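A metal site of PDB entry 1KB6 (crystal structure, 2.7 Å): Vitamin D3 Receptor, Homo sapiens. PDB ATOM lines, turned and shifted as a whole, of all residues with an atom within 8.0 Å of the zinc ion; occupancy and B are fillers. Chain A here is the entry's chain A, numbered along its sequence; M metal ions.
N of Phe 47 lies close to SG of Cys 45, 3.4 Å away.
The side-chain sulfur (SG) of Cys 45 lies close to the backbone NH (N) of Gly 49, 3.0 Å away.
N of Asn 48 lies close to SG of Cys 45 (3.7 Å).
N of Asp 50 lies close to SG of Cys 64 (3.5 Å).
Four residues have an atom within 4 Å of the zinc ion: Cys 45, Cys 51, Cys 61 and Cys 64.
The nearest printed residue that does not touch the zinc ion is Gly 49 (4.2 Å).
The zinc ion is bound by SG of Cys 45 (2.2 Å), SG of Cys 64 (2.2 Å), SG of Cys 61 (2.3 Å) and SG of Cys 51 (2.3 Å).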
ATOM      1  N   THR A  44      19.247 -19.178  -3.251  1.00  0.00           N
ATOM      2  CA  THR A  44      19.573 -20.538  -2.778  1.00  0.00           C
ATOM      3  C   THR A  44      19.609 -21.549  -3.941  1.00  0.00           C
ATOM      4  O   THR A  44      18.756 -21.519  -4.841  1.00  0.00           O
ATOM      5  CB  THR A  44      18.584 -21.044  -1.716  1.00  0.00           C
ATOM      6  OG1 THR A  44      17.512 -21.730  -2.384  1.00  0.00           O
ATOM      7  CG2 THR A  44      18.027 -19.874  -0.891  1.00  0.00           C
ATOM      8  N   CYS A  45      20.591 -22.440  -3.923  1.00  0.00           N
ATOM      9  CA  CYS A  45      20.676 -23.375  -5.018  1.00  0.00           C
ATOM     10  C   CYS A  45      19.578 -24.402  -4.962  1.00  0.00           C
ATOM     11  O   CYS A  45      19.392 -25.048  -3.967  1.00  0.00           O
ATOM     12  CB  CYS A  45      22.021 -24.074  -5.012  1.00  0.00           C
ATOM     13  SG  CYS A  45      22.381 -24.816  -6.562  1.00  0.00           S
ATOM     14  N   PRO A  46      18.823 -24.553  -6.041  1.00  0.00           N
ATOM     15  CA  PRO A  46      17.794 -25.570  -5.923  1.00  0.00           C
ATOM     16  C   PRO A  46      18.415 -26.923  -6.308  1.00  0.00           C
ATOM     17  O   PRO A  46      17.691 -27.865  -6.576  1.00  0.00           O
ATOM     18  CB  PRO A  46      16.785 -25.105  -6.953  1.00  0.00           C
ATOM     19  CG  PRO A  46      17.684 -24.648  -8.078  1.00  0.00           C
ATOM     20  CD  PRO A  46      18.723 -23.850  -7.326  1.00  0.00           C
ATOM     21  N   PHE A  47      19.743 -26.990  -6.358  1.00  0.00           N
ATOM     22  CA  PHE A  47      20.473 -28.215  -6.730  1.00  0.00           C
ATOM     23  C   PHE A  47      21.564 -28.625  -5.726  1.00  0.00           C
ATOM     24  O   PHE A  47      21.235 -29.083  -4.651  1.00  0.00           O
ATOM     25  CB  PHE A  47      21.076 -28.053  -8.112  1.00  0.00           C
ATOM     26  CG  PHE A  47      20.050 -27.953  -9.208  1.00  0.00           C
ATOM     27  CD1 PHE A  47      19.264 -29.043  -9.553  1.00  0.00           C
ATOM     28  CD2 PHE A  47      19.901 -26.790  -9.922  1.00  0.00           C
ATOM     29  CE1 PHE A  47      18.352 -28.967 -10.597  1.00  0.00           C
ATOM     30  CE2 PHE A  47      18.986 -26.710 -10.975  1.00  0.00           C
ATOM     31  CZ  PHE A  47      18.211 -27.799 -11.312  1.00  0.00           C
ATOM     32  N   ASN A  48      22.851 -28.442  -6.046  1.00  0.00           N
ATOM     33  CA  ASN A  48      23.890 -28.830  -5.095  1.00  0.00           C
ATOM     34  C   ASN A  48      24.823 -27.707  -4.728  1.00  0.00           C
ATOM     35  O   ASN A  48      25.800 -27.921  -3.984  1.00  0.00           O
ATOM     36  CB  ASN A  48      24.746 -29.967  -5.646  1.00  0.00           C
ATOM     37  CG  ASN A  48      23.933 -31.116  -6.120  1.00  0.00           C
ATOM     38  OD1 ASN A  48      23.199 -31.720  -5.349  1.00  0.00           O
ATOM     39  ND2 ASN A  48      24.048 -31.427  -7.387  1.00  0.00           N
ATOM     40  N   GLY A  49      24.545 -26.518  -5.250  1.00  0.00           N
ATOM     41  CA  GLY A  49      25.366 -25.390  -4.909  1.00  0.00           C
ATOM     42  C   GLY A  49      26.752 -25.503  -5.458  1.00  0.00           C
ATOM     43  O   GLY A  49      27.742 -25.224  -4.781  1.00  0.00           O
ATOM     44  N   ASP A  50      26.828 -25.971  -6.697  1.00  0.00           N
ATOM     45  CA  ASP A  50      28.068 -26.093  -7.445  1.00  0.00           C
ATOM     46  C   ASP A  50      27.681 -26.210  -8.896  1.00  0.00           C
ATOM     47  O   ASP A  50      28.217 -27.026  -9.599  1.00  0.00           O
ATOM     48  CB  ASP A  50      28.872 -27.309  -6.994  1.00  0.00           C
ATOM     49  CG  ASP A  50      28.143 -28.572  -7.214  1.00  0.00           C
ATOM     50  OD1 ASP A  50      27.013 -28.516  -7.745  1.00  0.00           O
ATOM     51  OD2 ASP A  50      28.692 -29.621  -6.876  1.00  0.00           O
ATOM     52  N   CYS A  51      26.725 -25.403  -9.337  1.00  0.00           N
ATOM     53  CA  CYS A  51      26.285 -25.414 -10.713  1.00  0.00           C
ATOM     54  C   CYS A  51      27.394 -24.900 -11.614  1.00  0.00           C
ATOM     55  O   CYS A  51      28.227 -24.099 -11.200  1.00  0.00           O
ATOM     56  CB  CYS A  51      25.032 -24.540 -10.912  1.00  0.00           C
ATOM     57  SG  CYS A  51      23.484 -24.985 -10.035  1.00  0.00           S
ATOM     58  N   ARG A  52      27.442 -25.399 -12.835  1.00  0.00           N
ATOM     59  CA  ARG A  52      28.444 -24.962 -13.795  1.00  0.00           C
ATOM     60  C   ARG A  52      27.709 -23.876 -14.626  1.00  0.00           C
ATOM     61  O   ARG A  52      26.809 -24.171 -15.393  1.00  0.00           O
ATOM     62  CB  ARG A  52      28.934 -26.175 -14.618  1.00  0.00           C
ATOM     63  CG  ARG A  52      29.836 -27.134 -13.818  1.00  0.00           C
ATOM     64  CD  ARG A  52      30.261 -28.388 -14.530  1.00  0.00           C
ATOM     65  NE  ARG A  52      31.471 -29.009 -13.980  1.00  0.00           N
ATOM     66  CZ  ARG A  52      32.194 -29.947 -14.627  1.00  0.00           C
ATOM     67  NH1 ARG A  52      31.820 -30.362 -15.823  1.00  0.00           N
ATOM     68  NH2 ARG A  52      33.284 -30.494 -14.088  1.00  0.00           N
ATOM     69  N   ILE A  53      28.082 -22.617 -14.453  1.00  0.00           N
ATOM     70  CA  ILE A  53      27.352 -21.568 -15.139  1.00  0.00           C
ATOM     71  C   ILE A  53      27.761 -21.477 -16.568  1.00  0.00           C
ATOM     72  O   ILE A  53      28.921 -21.577 -16.893  1.00  0.00           O
ATOM     73  CB  ILE A  53      27.605 -20.166 -14.439  1.00  0.00           C
ATOM     74  CG1 ILE A  53      27.710 -20.363 -12.915  1.00  0.00           C
ATOM     75  CG2 ILE A  53      26.441 -19.209 -14.675  1.00  0.00           C
ATOM     76  CD1 ILE A  53      26.511 -21.036 -12.338  1.00  0.00           C
ATOM     77  N   HIS A  60      19.106 -19.390 -14.815  1.00  0.00           N
ATOM     78  CA  HIS A  60      18.520 -20.207 -13.771  1.00  0.00           C
ATOM     79  C   HIS A  60      19.138 -20.325 -12.411  1.00  0.00           C
ATOM     80  O   HIS A  60      18.435 -20.155 -11.437  1.00  0.00           O
ATOM     81  CB  HIS A  60      18.161 -21.582 -14.297  1.00  0.00           C
ATOM     82  CG  HIS A  60      16.962 -21.570 -15.195  1.00  0.00           C
ATOM     83  ND1 HIS A  60      15.739 -21.037 -14.809  1.00  0.00           N
ATOM     84  CD2 HIS A  60      16.804 -21.940 -16.496  1.00  0.00           C
ATOM     85  CE1 HIS A  60      14.898 -21.070 -15.818  1.00  0.00           C
ATOM     86  NE2 HIS A  60      15.514 -21.608 -16.857  1.00  0.00           N
ATOM     87  N   CYS A  61      20.414 -20.630 -12.245  1.00  0.00           N
ATOM     88  CA  CYS A  61      20.770 -20.653 -10.855  1.00  0.00           C
ATOM     89  C   CYS A  61      21.379 -19.324 -10.472  1.00  0.00           C
ATOM     90  O   CYS A  61      22.546 -19.026 -10.745  1.00  0.00           O
ATOM     91  CB  CYS A  61      21.692 -21.834 -10.466  1.00  0.00           C
ATOM     92  SG  CYS A  61      21.972 -21.935  -8.648  1.00  0.00           S
ATOM     93  N   GLN A  62      20.580 -18.508  -9.800  1.00  0.00           N
ATOM     94  CA  GLN A  62      21.089 -17.222  -9.366  1.00  0.00           C
ATOM     95  C   GLN A  62      22.072 -17.346  -8.220  1.00  0.00           C
ATOM     96  O   GLN A  62      23.088 -16.648  -8.167  1.00  0.00           O
ATOM     97  CB  GLN A  62      19.925 -16.357  -8.984  1.00  0.00           C
ATOM     98  CG  GLN A  62      18.901 -16.331 -10.035  1.00  0.00           C
ATOM     99  CD  GLN A  62      17.739 -15.503  -9.637  1.00  0.00           C
ATOM    100  OE1 GLN A  62      17.068 -15.768  -8.617  1.00  0.00           O
ATOM    101  NE2 GLN A  62      17.449 -14.478 -10.431  1.00  0.00           N
ATOM    102  N   ALA A  63      21.750 -18.229  -7.298  1.00  0.00           N
ATOM    103  CA  ALA A  63      22.604 -18.466  -6.162  1.00  0.00           C
ATOM    104  C   ALA A  63      24.014 -18.665  -6.598  1.00  0.00           C
ATOM    105  O   ALA A  63      24.915 -17.916  -6.189  1.00  0.00           O
ATOM    106  CB  ALA A  63      22.149 -19.674  -5.456  1.00  0.00           C
ATOM    107  N   CYS A  64      24.221 -19.665  -7.451  1.00  0.00           N
ATOM    108  CA  CYS A  64      25.549 -20.034  -7.933  1.00  0.00           C
ATOM    109  C   CYS A  64      26.146 -18.985  -8.812  1.00  0.00           C
ATOM    110  O   CYS A  64      27.333 -18.694  -8.692  1.00  0.00           O
ATOM    111  CB  CYS A  64      25.523 -21.385  -8.680  1.00  0.00           C
ATOM    112  SG  CYS A  64      25.340 -22.900  -7.643  1.00  0.00           S
ATOM    113  N   ARG A  65      25.336 -18.411  -9.693  1.00  0.00           N
ATOM    114  CA  ARG A  65      25.844 -17.350 -10.532  1.00  0.00           C
ATOM    115  C   ARG A  65      26.376 -16.256  -9.623  1.00  0.00           C
ATOM    116  O   ARG A  65      27.455 -15.763  -9.821  1.00  0.00           O
ATOM    117  CB  ARG A  65      24.736 -16.797 -11.406  1.00  0.00           C
ATOM    118  CG  ARG A  65      25.147 -15.664 -12.325  1.00  0.00           C
ATOM    119  CD  ARG A  65      24.011 -15.346 -13.264  1.00  0.00           C
ATOM    120  NE  ARG A  65      24.486 -14.508 -14.351  1.00  0.00           N
ATOM    121  CZ  ARG A  65      23.720 -13.837 -15.233  1.00  0.00           C
ATOM    122  NH1 ARG A  65      22.382 -13.866 -15.194  1.00  0.00           N
ATOM    123  NH2 ARG A  65      24.307 -13.069 -16.137  1.00  0.00           N
HETATM  124 ZN    ZN M   1      23.332 -23.676  -8.159  1.00  0.00          ZN
